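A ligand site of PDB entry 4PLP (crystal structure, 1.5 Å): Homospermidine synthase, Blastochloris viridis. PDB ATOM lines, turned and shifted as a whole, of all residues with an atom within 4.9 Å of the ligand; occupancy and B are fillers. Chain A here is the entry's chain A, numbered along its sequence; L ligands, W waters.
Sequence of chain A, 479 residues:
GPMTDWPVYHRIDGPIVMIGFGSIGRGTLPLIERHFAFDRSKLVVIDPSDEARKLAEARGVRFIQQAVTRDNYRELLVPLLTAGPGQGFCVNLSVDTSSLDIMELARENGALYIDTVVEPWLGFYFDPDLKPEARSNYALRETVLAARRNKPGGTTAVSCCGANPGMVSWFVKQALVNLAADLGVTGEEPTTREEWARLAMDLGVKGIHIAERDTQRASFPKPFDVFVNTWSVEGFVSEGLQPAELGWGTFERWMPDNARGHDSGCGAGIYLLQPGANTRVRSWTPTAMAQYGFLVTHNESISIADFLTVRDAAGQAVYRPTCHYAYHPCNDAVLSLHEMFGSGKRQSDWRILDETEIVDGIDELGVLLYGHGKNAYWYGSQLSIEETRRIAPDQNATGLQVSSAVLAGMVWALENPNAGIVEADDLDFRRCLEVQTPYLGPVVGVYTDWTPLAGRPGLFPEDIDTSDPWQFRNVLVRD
The backbone carbonyl oxygen (O) of Val 95 sits close to a nitrogen (N2) of the ligand, 3.0 Å away.
Residues that only touch the ligand: Ile 19, Phe 21, Gly 22, Pro 48, Ser 49, Ala 67, Leu 93, Thr 97, Val 117, Gly 162, Trp 231, Gly 235, Ile 352 and Val 402.
Water W5 lies within hydrogen-bond range of an oxygen (O8) of the ligand (2.7 Å), the backbone carbonyl oxygen (O) of Leu 93 (2.8 Å), the backbone NH (N) of Gly 22 (2.8 Å) and the backbone NH (N) of Gly 25 (3.0 Å).
Water W1 bridges N2 of the ligand and OD2 of Asp 96.
Water W8 lies within hydrogen-bond range of an oxygen (O2) of the ligand, the backbone NH (N) of Val 233 and the backbone NH (N) of Glu 234.
Water W7 bridges the side-chain carboxylate of Glu 234 and an oxygen (O2) of the ligand.
Water W10 bridges OE1 of Glu 119 (2.7 Å) and O13 of the ligand (3.0 Å).
OD1 of Asp 47 is in hydrogen-bond range of N of Ser 49, at 2.9 Å.
The side-chain carboxylate (OD2) of Asp 47 sits at hydrogen-bond distance from the backbone NH (N) of Phe 21 (2.7 Å).
OG of Ser 232 is in hydrogen-bond range of N of Gly 235, at 2.8 Å.
The side-chain hydroxyl of Ser 94 lies within hydrogen-bond range of the side-chain hydroxyl of Thr 97, 2.7 Å away.
N of Ser 94 lies within hydrogen-bond range of O of Ile 19 (3.3 Å).
N of Leu 93 lies within hydrogen-bond range of O of Ile 19.
OG of Ser 49 is in hydrogen-bond range of N of Ala 52 (3.0 Å).
O5 of the ligand lies within hydrogen-bond range of OD2 of Asp 47, 2.6 Å away.
An oxygen (O1) of the ligand lies within hydrogen-bond range of the backbone NH (N) of Ser 23, 2.9 Å away.
OG of Ser 23 lies within hydrogen-bond range of O9 of the ligand (2.7 Å).
The backbone NH (N) of Ser 232 sits at hydrogen-bond distance from an oxygen (O9) of the ligand.
The side-chain hydroxyl (OG) of Ser 232 sits at hydrogen-bond distance from an oxygen (O2) of the ligand, 2.8 Å away.
An oxygen (O8) of the ligand is in hydrogen-bond range of the backbone NH (N) of Ile 24 (2.9 Å).
O14 of the ligand lies within hydrogen-bond range of N of Asn 164 (2.9 Å).
O of Asn 164 lies close to N7 of the ligand.
O of Thr 116 sits at hydrogen-bond distance from N7 of the ligand, at 3.1 Å.
The side-chain hydroxyl of Thr 116 lies within hydrogen-bond range of an oxygen (O11) of the ligand.
The backbone NH (N) of Val 68 sits at hydrogen-bond distance from a nitrogen (N4) of the ligand (3.0 Å).
N3 of the ligand is in hydrogen-bond range of O of Val 68, 3.0 Å away.
The backbone carbonyl oxygen (O) of Ser 94 is in hydrogen-bond range of an oxygen (O12) of the ligand, 3.0 Å away.
An oxygen (O14) of the ligand lies within hydrogen-bond range of the backbone NH (N) of Ala 163 (3.0 Å).
The backbone carbonyl oxygen of Pro 165 sits at hydrogen-bond distance from a nitrogen (N7) of the ligand (3.1 Å).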
ATOM      1  N   ILE A  19     -25.196  -1.229  -9.394  1.00  0.00           N
ATOM      2  CA  ILE A  19     -25.879  -2.322 -10.031  1.00  0.00           C
ATOM      3  C   ILE A  19     -24.859  -3.188 -10.792  1.00  0.00           C
ATOM      4  O   ILE A  19     -24.212  -2.720 -11.732  1.00  0.00           O
ATOM      5  CB  ILE A  19     -26.994  -1.838 -10.942  1.00  0.00           C
ATOM      6  CG1 ILE A  19     -27.867  -0.791 -10.210  1.00  0.00           C
ATOM      7  CG2 ILE A  19     -27.817  -2.997 -11.431  1.00  0.00           C
ATOM      8  CD1 ILE A  19     -29.019  -0.300 -11.063  1.00  0.00           C
ATOM      9  N   GLY A  20     -24.711  -4.429 -10.350  1.00  0.00           N
ATOM     10  CA  GLY A  20     -23.741  -5.345 -10.908  1.00  0.00           C
ATOM     11  C   GLY A  20     -22.424  -5.366 -10.173  1.00  0.00           C
ATOM     12  O   GLY A  20     -21.836  -4.332  -9.865  1.00  0.00           O
ATOM     13  N   PHE A  21     -21.922  -6.566  -9.887  1.00  0.00           N
ATOM     14  CA  PHE A  21     -20.680  -6.737  -9.150  1.00  0.00           C
ATOM     15  C   PHE A  21     -19.923  -7.878  -9.809  1.00  0.00           C
ATOM     16  O   PHE A  21     -19.572  -8.857  -9.157  1.00  0.00           O
ATOM     17  CB  PHE A  21     -20.988  -7.080  -7.700  1.00  0.00           C
ATOM     18  CG  PHE A  21     -19.854  -6.858  -6.733  1.00  0.00           C
ATOM     19  CD1 PHE A  21     -19.255  -5.621  -6.654  1.00  0.00           C
ATOM     20  CD2 PHE A  21     -19.455  -7.863  -5.860  1.00  0.00           C
ATOM     21  CE1 PHE A  21     -18.230  -5.393  -5.776  1.00  0.00           C
ATOM     22  CE2 PHE A  21     -18.427  -7.662  -4.947  1.00  0.00           C
ATOM     23  CZ  PHE A  21     -17.798  -6.403  -4.904  1.00  0.00           C
ATOM     24  N   GLY A  22     -19.751  -7.737 -11.117  1.00  0.00           N
ATOM     25  CA  GLY A  22     -18.887  -8.606 -11.896  1.00  0.00           C
ATOM     26  C   GLY A  22     -17.466  -8.051 -11.954  1.00  0.00           C
ATOM     27  O   GLY A  22     -17.006  -7.414 -11.002  1.00  0.00           O
ATOM     28  N   SER A  23     -16.773  -8.263 -13.076  1.00  0.00           N
ATOM     29  CA  SER A  23     -15.343  -7.910 -13.110  1.00  0.00           C
ATOM     30  C   SER A  23     -15.188  -6.421 -12.937  1.00  0.00           C
ATOM     31  O   SER A  23     -14.265  -5.994 -12.265  1.00  0.00           O
ATOM     32  CB  SER A  23     -14.635  -8.462 -14.381  1.00  0.00           C
ATOM     33  OG  SER A  23     -14.709  -7.598 -15.496  1.00  0.00           O
ATOM     34  N   ILE A  24     -16.077  -5.620 -13.470  1.00  0.00           N
ATOM     35  CA  ILE A  24     -15.883  -4.160 -13.402  1.00  0.00           C
ATOM     36  C   ILE A  24     -16.394  -3.610 -12.063  1.00  0.00           C
ATOM     37  O   ILE A  24     -15.742  -2.747 -11.445  1.00  0.00           O
ATOM     38  CB  ILE A  24     -16.569  -3.429 -14.586  1.00  0.00           C
ATOM     39  CG1 ILE A  24     -16.024  -3.895 -15.953  1.00  0.00           C
ATOM     40  CG2 ILE A  24     -16.265  -1.912 -14.516  1.00  0.00           C
ATOM     41  CD1 ILE A  24     -14.492  -4.026 -16.014  1.00  0.00           C
ATOM     42  N   GLY A  25     -17.552  -4.078 -11.606  1.00  0.00           N
ATOM     43  CA  GLY A  25     -18.044  -3.629 -10.297  1.00  0.00           C
ATOM     44  C   GLY A  25     -17.046  -3.920  -9.197  1.00  0.00           C
ATOM     45  O   GLY A  25     -16.744  -3.087  -8.381  1.00  0.00           O
ATOM     46  N   ILE A  46     -26.082  -4.376  -5.871  1.00  0.00           N
ATOM     47  CA  ILE A  46     -27.181  -5.248  -6.263  1.00  0.00           C
ATOM     48  C   ILE A  46     -26.730  -6.152  -7.408  1.00  0.00           C
ATOM     49  O   ILE A  46     -26.313  -5.667  -8.483  1.00  0.00           O
ATOM     50  CB  ILE A  46     -28.387  -4.467  -6.771  1.00  0.00           C
ATOM     51  CG1 ILE A  46     -28.760  -3.344  -5.820  1.00  0.00           C
ATOM     52  CG2 ILE A  46     -29.541  -5.365  -7.009  1.00  0.00           C
ATOM     53  CD1 ILE A  46     -29.845  -2.426  -6.389  1.00  0.00           C
ATOM     54  N   ASP A  47     -26.854  -7.471  -7.200  1.00  0.00           N
ATOM     55  CA  ASP A  47     -26.403  -8.463  -8.187  1.00  0.00           C
ATOM     56  C   ASP A  47     -27.016  -9.845  -7.832  1.00  0.00           C
ATOM     57  O   ASP A  47     -26.971 -10.259  -6.686  1.00  0.00           O
ATOM     58  CB  ASP A  47     -24.871  -8.528  -8.168  1.00  0.00           C
ATOM     59  CG  ASP A  47     -24.286  -9.358  -9.316  1.00  0.00           C
ATOM     60  OD1 ASP A  47     -24.665 -10.547  -9.471  1.00  0.00           O
ATOM     61  OD2 ASP A  47     -23.445  -8.831 -10.101  1.00  0.00           O
ATOM     62  N   PRO A  48     -27.541 -10.551  -8.843  1.00  0.00           N
ATOM     63  CA  PRO A  48     -28.216 -11.836  -8.550  1.00  0.00           C
ATOM     64  C   PRO A  48     -27.304 -13.013  -8.238  1.00  0.00           C
ATOM     65  O   PRO A  48     -27.775 -14.060  -7.779  1.00  0.00           O
ATOM     66  CB  PRO A  48     -29.003 -12.123  -9.844  1.00  0.00           C
ATOM     67  CG  PRO A  48     -28.273 -11.383 -10.903  1.00  0.00           C
ATOM     68  CD  PRO A  48     -27.738 -10.126 -10.236  1.00  0.00           C
ATOM     69  N   SER A  49     -26.007 -12.847  -8.453  1.00  0.00           N
ATOM     70  CA  SER A  49     -25.066 -13.973  -8.364  1.00  0.00           C
ATOM     71  C   SER A  49     -24.607 -14.346  -6.957  1.00  0.00           C
ATOM     72  O   SER A  49     -24.209 -13.498  -6.166  1.00  0.00           O
ATOM     73  CB  SER A  49     -23.847 -13.648  -9.221  1.00  0.00           C
ATOM     74  OG  SER A  49     -22.704 -14.309  -8.729  1.00  0.00           O
ATOM     75  N   ALA A  52     -20.882 -13.373  -6.501  1.00  0.00           N
ATOM     76  CA  ALA A  52     -20.758 -11.950  -6.195  1.00  0.00           C
ATOM     77  C   ALA A  52     -21.112 -11.707  -4.716  1.00  0.00           C
ATOM     78  O   ALA A  52     -20.430 -10.952  -4.031  1.00  0.00           O
ATOM     79  CB  ALA A  52     -21.639 -11.114  -7.100  1.00  0.00           C
ATOM     80  N   GLN A  66     -30.385  -9.685  -5.975  1.00  0.00           N
ATOM     81  CA  GLN A  66     -31.570  -9.528  -6.778  1.00  0.00           C
ATOM     82  C   GLN A  66     -31.142  -9.164  -8.204  1.00  0.00           C
ATOM     83  O   GLN A  66     -30.118  -8.503  -8.420  1.00  0.00           O
ATOM     84  CB  GLN A  66     -32.436  -8.444  -6.120  1.00  0.00           C
ATOM     85  CG  GLN A  66     -33.897  -8.492  -6.438  1.00  0.00           C
ATOM     86  CD  GLN A  66     -34.523  -9.794  -6.013  1.00  0.00           C
ATOM     87  OE1 GLN A  66     -34.415 -10.202  -4.851  1.00  0.00           O
ATOM     88  NE2 GLN A  66     -35.125 -10.479  -6.952  1.00  0.00           N
ATOM     89  N   ALA A  67     -31.908  -9.631  -9.175  1.00  0.00           N
ATOM     90  CA  ALA A  67     -31.757  -9.225 -10.564  1.00  0.00           C
ATOM     91  C   ALA A  67     -32.691  -8.051 -10.780  1.00  0.00           C
ATOM     92  O   ALA A  67     -33.871  -8.134 -10.453  1.00  0.00           O
ATOM     93  CB  ALA A  67     -32.132 -10.366 -11.500  1.00  0.00           C
ATOM     94  N   VAL A  68     -32.177  -6.949 -11.311  1.00  0.00           N
ATOM     95  CA  VAL A  68     -33.021  -5.821 -11.668  1.00  0.00           C
ATOM     96  C   VAL A  68     -33.696  -6.090 -13.002  1.00  0.00           C
ATOM     97  O   VAL A  68     -33.034  -6.383 -13.988  1.00  0.00           O
ATOM     98  CB  VAL A  68     -32.164  -4.542 -11.746  1.00  0.00           C
ATOM     99  CG1 VAL A  68     -33.003  -3.356 -12.131  1.00  0.00           C
ATOM    100  CG2 VAL A  68     -31.496  -4.301 -10.405  1.00  0.00           C
ATOM    101  N   LEU A  93     -23.150  -1.049 -13.635  1.00  0.00           N
ATOM    102  CA  LEU A  93     -22.093  -1.919 -14.158  1.00  0.00           C
ATOM    103  C   LEU A  93     -22.594  -3.322 -14.408  1.00  0.00           C
ATOM    104  O   LEU A  93     -21.897  -4.304 -14.148  1.00  0.00           O
ATOM    105  CB  LEU A  93     -20.914  -1.917 -13.172  1.00  0.00           C
ATOM    106  CG  LEU A  93     -20.389  -0.508 -12.874  1.00  0.00           C
ATOM    107  CD1 LEU A  93     -19.319  -0.551 -11.813  1.00  0.00           C
ATOM    108  CD2 LEU A  93     -19.869   0.196 -14.143  1.00  0.00           C
ATOM    109  N   SER A  94     -23.803  -3.438 -14.951  1.00  0.00           N
ATOM    110  CA  SER A  94     -24.454  -4.743 -15.084  1.00  0.00           C
ATOM    111  C   SER A  94     -24.592  -5.163 -16.556  1.00  0.00           C
ATOM    112  O   SER A  94     -24.238  -4.429 -17.488  1.00  0.00           O
ATOM    113  CB  SER A  94     -25.831  -4.645 -14.430  1.00  0.00           C
ATOM    114  OG  SER A  94     -26.585  -3.658 -15.102  1.00  0.00           O
ATOM    115  N   VAL A  95     -25.042  -6.392 -16.748  1.00  0.00           N
ATOM    116  CA  VAL A  95     -25.616  -6.826 -18.015  1.00  0.00           C
ATOM    117  C   VAL A  95     -27.111  -7.094 -17.837  1.00  0.00           C
ATOM    118  O   VAL A  95     -27.601  -7.265 -16.698  1.00  0.00           O
ATOM    119  CB  VAL A  95     -24.930  -8.106 -18.522  1.00  0.00           C
ATOM    120  CG1 VAL A  95     -23.405  -7.844 -18.810  1.00  0.00           C
ATOM    121  CG2 VAL A  95     -25.115  -9.251 -17.544  1.00  0.00           C
ATOM    122  N   ASP A  96     -27.793  -7.112 -18.981  1.00  0.00           N
ATOM    123  CA  ASP A  96     -29.195  -7.538 -19.114  1.00  0.00           C
ATOM    124  C   ASP A  96     -30.171  -6.504 -18.561  1.00  0.00           C
ATOM    125  O   ASP A  96     -31.341  -6.800 -18.441  1.00  0.00           O
ATOM    126  CB  ASP A  96     -29.416  -8.906 -18.460  1.00  0.00           C
ATOM    127  CG  ASP A  96     -28.681 -10.034 -19.194  1.00  0.00           C
ATOM    128  OD1 ASP A  96     -28.329  -9.843 -20.379  1.00  0.00           O
ATOM    129  OD2 ASP A  96     -28.457 -11.083 -18.569  1.00  0.00           O
ATOM    130  N   THR A  97     -29.691  -5.308 -18.255  1.00  0.00           N
ATOM    131  CA  THR A  97     -30.545  -4.247 -17.781  1.00  0.00           C
ATOM    132  C   THR A  97     -30.634  -3.099 -18.765  1.00  0.00           C
ATOM    133  O   THR A  97     -29.694  -2.854 -19.527  1.00  0.00           O
ATOM    134  CB  THR A  97     -30.012  -3.689 -16.482  1.00  0.00           C
ATOM    135  OG1 THR A  97     -28.713  -3.145 -16.726  1.00  0.00           O
ATOM    136  CG2 THR A  97     -29.916  -4.747 -15.440  1.00  0.00           C
ATOM    137  N   THR A 116     -21.434   2.116 -18.516  1.00  0.00           N
ATOM    138  CA  THR A 116     -20.331   1.897 -19.437  1.00  0.00           C
ATOM    139  C   THR A 116     -20.779   1.350 -20.802  1.00  0.00           C
ATOM    140  O   THR A 116     -19.958   0.988 -21.637  1.00  0.00           O
ATOM    141  CB  THR A 116     -19.341   0.893 -18.842  1.00  0.00           C
ATOM    142  OG1 THR A 116     -20.011  -0.342 -18.641  1.00  0.00           O
ATOM    143  CG2 THR A 116     -18.761   1.414 -17.530  1.00  0.00           C
ATOM    144  N   VAL A 117     -22.078   1.306 -21.015  1.00  0.00           N
ATOM    145  CA  VAL A 117     -22.605   0.713 -22.234  1.00  0.00           C
ATOM    146  C   VAL A 117     -24.074   1.068 -22.287  1.00  0.00           C
ATOM    147  O   VAL A 117     -24.702   1.223 -21.236  1.00  0.00           O
ATOM    148  CB  VAL A 117     -22.435  -0.817 -22.186  1.00  0.00           C
ATOM    149  CG1 VAL A 117     -23.196  -1.421 -20.967  1.00  0.00           C
ATOM    150  CG2 VAL A 117     -22.951  -1.477 -23.492  1.00  0.00           C
ATOM    151  N   GLU A 119     -27.131  -0.667 -22.684  1.00  0.00           N
ATOM    152  CA  GLU A 119     -27.595  -2.046 -22.622  1.00  0.00           C
ATOM    153  C   GLU A 119     -29.131  -2.030 -22.702  1.00  0.00           C
ATOM    154  O   GLU A 119     -29.779  -1.123 -22.171  1.00  0.00           O
ATOM    155  CB  GLU A 119     -27.134  -2.659 -21.283  1.00  0.00           C
ATOM    156  CG  GLU A 119     -27.426  -4.155 -21.054  1.00  0.00           C
ATOM    157  CD  GLU A 119     -26.400  -5.087 -21.691  1.00  0.00           C
ATOM    158  OE1 GLU A 119     -25.600  -4.612 -22.541  1.00  0.00           O
ATOM    159  OE2 GLU A 119     -26.423  -6.310 -21.359  1.00  0.00           O
ATOM    160  N   GLY A 162     -16.698   4.051 -19.820  1.00  0.00           N
ATOM    161  CA  GLY A 162     -15.700   3.065 -19.462  1.00  0.00           C
ATOM    162  C   GLY A 162     -14.362   3.357 -20.144  1.00  0.00           C
ATOM    163  O   GLY A 162     -13.982   4.515 -20.360  1.00  0.00           O
ATOM    164  N   ALA A 163     -13.610   2.325 -20.480  1.00  0.00           N
ATOM    165  CA  ALA A 163     -12.347   2.498 -21.203  1.00  0.00           C
ATOM    166  C   ALA A 163     -12.652   2.807 -22.649  1.00  0.00           C
ATOM    167  O   ALA A 163     -12.047   3.686 -23.289  1.00  0.00           O
ATOM    168  CB  ALA A 163     -11.471   1.241 -21.088  1.00  0.00           C
ATOM    169  N   ASN A 164     -13.563   2.015 -23.210  1.00  0.00           N
ATOM    170  CA  ASN A 164     -13.931   2.164 -24.594  1.00  0.00           C
ATOM    171  C   ASN A 164     -15.245   1.448 -24.797  1.00  0.00           C
ATOM    172  O   ASN A 164     -15.331   0.239 -24.733  1.00  0.00           O
ATOM    173  CB  ASN A 164     -12.828   1.684 -25.572  1.00  0.00           C
ATOM    174  CG  ASN A 164     -12.364   0.240 -25.337  1.00  0.00           C
ATOM    175  OD1 ASN A 164     -12.274  -0.255 -24.212  1.00  0.00           O
ATOM    176  ND2 ASN A 164     -12.047  -0.443 -26.429  1.00  0.00           N
ATOM    177  N   PRO A 165     -16.317   2.205 -24.952  1.00  0.00           N
ATOM    178  CA  PRO A 165     -16.410   3.658 -24.959  1.00  0.00           C
ATOM    179  C   PRO A 165     -16.075   4.287 -23.612  1.00  0.00           C
ATOM    180  O   PRO A 165     -16.191   3.638 -22.541  1.00  0.00           O
ATOM    181  CB  PRO A 165     -17.890   3.910 -25.256  1.00  0.00           C
ATOM    182  CG  PRO A 165     -18.574   2.669 -24.660  1.00  0.00           C
ATOM    183  CD  PRO A 165     -17.628   1.543 -25.045  1.00  0.00           C
ATOM    184  N   TRP A 231     -12.587  -9.767 -19.322  1.00  0.00           N
ATOM    185  CA  TRP A 231     -13.722  -8.991 -18.889  1.00  0.00           C
ATOM    186  C   TRP A 231     -14.982  -9.767 -19.336  1.00  0.00           C
ATOM    187  O   TRP A 231     -14.874 -10.888 -19.850  1.00  0.00           O
ATOM    188  CB  TRP A 231     -13.683  -7.600 -19.500  1.00  0.00           C
ATOM    189  CG  TRP A 231     -13.768  -7.558 -20.950  1.00  0.00           C
ATOM    190  CD1 TRP A 231     -12.765  -7.797 -21.839  1.00  0.00           C
ATOM    191  CD2 TRP A 231     -14.931  -7.239 -21.749  1.00  0.00           C
ATOM    192  NE1 TRP A 231     -13.214  -7.611 -23.132  1.00  0.00           N
ATOM    193  CE2 TRP A 231     -14.534  -7.256 -23.100  1.00  0.00           C
ATOM    194  CE3 TRP A 231     -16.244  -6.891 -21.432  1.00  0.00           C
ATOM    195  CZ2 TRP A 231     -15.422  -7.011 -24.153  1.00  0.00           C
ATOM    196  CZ3 TRP A 231     -17.123  -6.611 -22.465  1.00  0.00           C
ATOM    197  CH2 TRP A 231     -16.697  -6.674 -23.815  1.00  0.00           C
ATOM    198  N   SER A 232     -16.148  -9.181 -19.163  1.00  0.00           N
ATOM    199  CA  SER A 232     -17.429  -9.911 -19.300  1.00  0.00           C
ATOM    200  C   SER A 232     -17.449 -10.858 -20.470  1.00  0.00           C
ATOM    201  O   SER A 232     -17.228 -10.422 -21.602  1.00  0.00           O
ATOM    202  CB  SER A 232     -18.561  -8.909 -19.515  1.00  0.00           C
ATOM    203  OG  SER A 232     -19.802  -9.557 -19.477  1.00  0.00           O
ATOM    204  N   VAL A 233     -17.706 -12.154 -20.223  1.00  0.00           N
ATOM    205  CA  VAL A 233     -17.915 -13.050 -21.328  1.00  0.00           C
ATOM    206  C   VAL A 233     -19.289 -12.788 -21.932  1.00  0.00           C
ATOM    207  O   VAL A 233     -19.418 -12.657 -23.168  1.00  0.00           O
ATOM    208  CB  VAL A 233     -17.696 -14.512 -20.906  1.00  0.00           C
ATOM    209  CG1 VAL A 233     -18.225 -15.467 -21.969  1.00  0.00           C
ATOM    210  CG2 VAL A 233     -16.199 -14.763 -20.660  1.00  0.00           C
ATOM    211  N   GLU A 234     -20.306 -12.665 -21.082  1.00  0.00           N
ATOM    212  CA  GLU A 234     -21.650 -12.364 -21.595  1.00  0.00           C
ATOM    213  C   GLU A 234     -21.678 -11.068 -22.435  1.00  0.00           C
ATOM    214  O   GLU A 234     -22.237 -11.019 -23.507  1.00  0.00           O
ATOM    215  CB  GLU A 234     -22.683 -12.355 -20.463  1.00  0.00           C
ATOM    216  CG  GLU A 234     -23.057 -13.805 -20.043  1.00  0.00           C
ATOM    217  CD  GLU A 234     -23.848 -13.916 -18.738  1.00  0.00           C
ATOM    218  OE1 GLU A 234     -24.074 -12.896 -18.049  1.00  0.00           O
ATOM    219  OE2 GLU A 234     -24.240 -15.056 -18.388  1.00  0.00           O
ATOM    220  N   GLY A 235     -21.032 -10.014 -21.939  1.00  0.00           N
ATOM    221  CA  GLY A 235     -20.961  -8.751 -22.647  1.00  0.00           C
ATOM    222  C   GLY A 235     -20.209  -8.807 -23.954  1.00  0.00           C
ATOM    223  O   GLY A 235     -20.659  -8.238 -24.941  1.00  0.00           O
ATOM    224  N   TRP A 350     -17.791 -20.708 -19.019  1.00  0.00           N
ATOM    225  CA  TRP A 350     -16.932 -19.561 -19.292  1.00  0.00           C
ATOM    226  C   TRP A 350     -16.277 -19.095 -18.023  1.00  0.00           C
ATOM    227  O   TRP A 350     -16.698 -19.436 -16.915  1.00  0.00           O
ATOM    228  CB  TRP A 350     -17.716 -18.411 -19.897  1.00  0.00           C
ATOM    229  CG  TRP A 350     -18.893 -17.883 -19.092  1.00  0.00           C
ATOM    230  CD1 TRP A 350     -20.207 -18.199 -19.278  1.00  0.00           C
ATOM    231  CD2 TRP A 350     -18.869 -16.892 -18.041  1.00  0.00           C
ATOM    232  NE1 TRP A 350     -20.989 -17.486 -18.410  1.00  0.00           N
ATOM    233  CE2 TRP A 350     -20.195 -16.679 -17.642  1.00  0.00           C
ATOM    234  CE3 TRP A 350     -17.850 -16.163 -17.408  1.00  0.00           C
ATOM    235  CZ2 TRP A 350     -20.536 -15.772 -16.629  1.00  0.00           C
ATOM    236  CZ3 TRP A 350     -18.199 -15.267 -16.392  1.00  0.00           C
ATOM    237  CH2 TRP A 350     -19.527 -15.078 -16.016  1.00  0.00           C
ATOM    238  N   ILE A 352     -13.662 -15.569 -16.459  1.00  0.00           N
ATOM    239  CA  ILE A 352     -12.950 -14.325 -16.651  1.00  0.00           C
ATOM    240  C   ILE A 352     -11.664 -14.460 -15.866  1.00  0.00           C
ATOM    241  O   ILE A 352     -11.741 -14.855 -14.703  1.00  0.00           O
ATOM    242  CB  ILE A 352     -13.764 -13.159 -16.110  1.00  0.00           C
ATOM    243  CG1 ILE A 352     -15.010 -12.992 -16.969  1.00  0.00           C
ATOM    244  CG2 ILE A 352     -12.961 -11.876 -16.091  1.00  0.00           C
ATOM    245  CD1 ILE A 352     -16.056 -11.959 -16.434  1.00  0.00           C
ATOM    246  N   VAL A 402     -11.128   0.340 -17.292  1.00  0.00           N
ATOM    247  CA  VAL A 402     -12.540   0.633 -17.232  1.00  0.00           C
ATOM    248  C   VAL A 402     -12.935   1.319 -15.910  1.00  0.00           C
ATOM    249  O   VAL A 402     -13.577   2.380 -15.930  1.00  0.00           O
ATOM    250  CB  VAL A 402     -13.385  -0.633 -17.463  1.00  0.00           C
ATOM    251  CG1 VAL A 402     -14.894  -0.310 -17.441  1.00  0.00           C
ATOM    252  CG2 VAL A 402     -13.002  -1.263 -18.775  1.00  0.00           C
HETATM  253  P1  LIG L   1     -19.501  -9.452 -15.813  1.00  0.00           P
HETATM  254  O1  LIG L   1     -18.202  -9.815 -15.123  1.00  0.00           O
HETATM  255  O2  LIG L   1     -20.135 -10.425 -16.786  1.00  0.00           O
HETATM  256  O3  LIG L   1     -20.523  -9.044 -14.671  1.00  0.00           O
HETATM  257  C1  LIG L   1     -21.868  -8.687 -15.016  1.00  0.00           C
HETATM  258  C2  LIG L   1     -22.673  -8.730 -13.720  1.00  0.00           C
HETATM  259  O4  LIG L   1     -24.026  -8.355 -13.988  1.00  0.00           O
HETATM  260  C3  LIG L   1     -22.705 -10.149 -13.132  1.00  0.00           C
HETATM  261  O5  LIG L   1     -22.135 -10.222 -11.829  1.00  0.00           O
HETATM  262  C4  LIG L   1     -24.182 -10.541 -13.137  1.00  0.00           C
HETATM  263  O6  LIG L   1     -24.569 -11.436 -12.072  1.00  0.00           O
HETATM  264  C5  LIG L   1     -24.809  -9.145 -13.118  1.00  0.00           C
HETATM  265  N1  LIG L   1     -26.196  -9.124 -13.608  1.00  0.00           N
HETATM  266  C6  LIG L   1     -26.715  -9.874 -14.603  1.00  0.00           C
HETATM  267  N2  LIG L   1     -28.023  -9.562 -14.765  1.00  0.00           N
HETATM  268  C7  LIG L   1     -28.314  -8.612 -13.852  1.00  0.00           C
HETATM  269  C8  LIG L   1     -29.490  -7.866 -13.475  1.00  0.00           C
HETATM  270  N3  LIG L   1     -30.616  -8.091 -14.144  1.00  0.00           N
HETATM  271  N4  LIG L   1     -29.406  -6.973 -12.471  1.00  0.00           N
HETATM  272  C9  LIG L   1     -28.248  -6.756 -11.817  1.00  0.00           C
HETATM  273  N5  LIG L   1     -27.122  -7.403 -12.119  1.00  0.00           N
HETATM  274  C10 LIG L   1     -27.106  -8.326 -13.108  1.00  0.00           C
HETATM  275  O7  LIG L   1     -19.425  -8.090 -16.660  1.00  0.00           O
HETATM  276  P2  LIG L   1     -18.300  -6.930 -16.437  1.00  0.00           P
HETATM  277  O8  LIG L   1     -18.320  -6.498 -15.001  1.00  0.00           O
HETATM  278  O9  LIG L   1     -16.980  -7.418 -16.926  1.00  0.00           O
HETATM  279  O10 LIG L   1     -18.819  -5.778 -17.431  1.00  0.00           O
HETATM  280  C11 LIG L   1     -19.903  -4.983 -16.896  1.00  0.00           C
HETATM  281  C12 LIG L   1     -20.582  -4.173 -17.968  1.00  0.00           C
HETATM  282  O11 LIG L   1     -19.651  -3.239 -18.481  1.00  0.00           O
HETATM  283  C13 LIG L   1     -20.985  -5.043 -19.139  1.00  0.00           C
HETATM  284  O12 LIG L   1     -22.233  -4.618 -19.673  1.00  0.00           O
HETATM  285  C14 LIG L   1     -19.909  -4.845 -20.154  1.00  0.00           C
HETATM  286  O13 LIG L   1     -20.346  -4.976 -21.514  1.00  0.00           O
HETATM  287  C15 LIG L   1     -19.455  -3.416 -19.863  1.00  0.00           C
HETATM  288  N6  LIG L   1     -18.057  -3.143 -20.138  1.00  0.00           N
HETATM  289  C16 LIG L   1     -17.771  -1.956 -20.711  1.00  0.00           C
HETATM  290  C17 LIG L   1     -16.467  -1.631 -21.036  1.00  0.00           C
HETATM  291  C18 LIG L   1     -16.057  -0.314 -21.624  1.00  0.00           C
HETATM  292  O14 LIG L   1     -14.859  -0.099 -21.714  1.00  0.00           O
HETATM  293  N7  LIG L   1     -16.918   0.677 -21.876  1.00  0.00           N
HETATM  294  C19 LIG L   1     -15.468  -2.549 -20.715  1.00  0.00           C
HETATM  295  C20 LIG L   1     -15.767  -3.704 -20.025  1.00  0.00           C
HETATM  296  C21 LIG L   1     -17.089  -3.970 -19.727  1.00  0.00           C
HETATM  297  O   HOH W   1     -29.831 -11.156 -16.110  1.00  0.00           O
HETATM  298  O   HOH W   2     -25.211 -13.830 -13.017  1.00  0.00           O
HETATM  299  O   HOH W   3     -32.322 -10.376 -15.570  1.00  0.00           O
HETATM  300  O   HOH W   4     -20.176 -12.128 -11.678  1.00  0.00           O
HETATM  301  O   HOH W   5     -19.750  -5.552 -12.946  1.00  0.00           O
HETATM  302  O   HOH W   6     -17.783 -11.792 -13.208  1.00  0.00           O
HETATM  303  O   HOH W   7     -22.337 -12.136 -16.037  1.00  0.00           O
HETATM  304  O   HOH W   8     -19.548 -12.795 -18.092  1.00  0.00           O
HETATM  305  O   HOH W   9     -19.427  -3.334 -23.655  1.00  0.00           O
HETATM  306  O   HOH W  10     -23.088  -5.627 -22.498  1.00  0.00           O
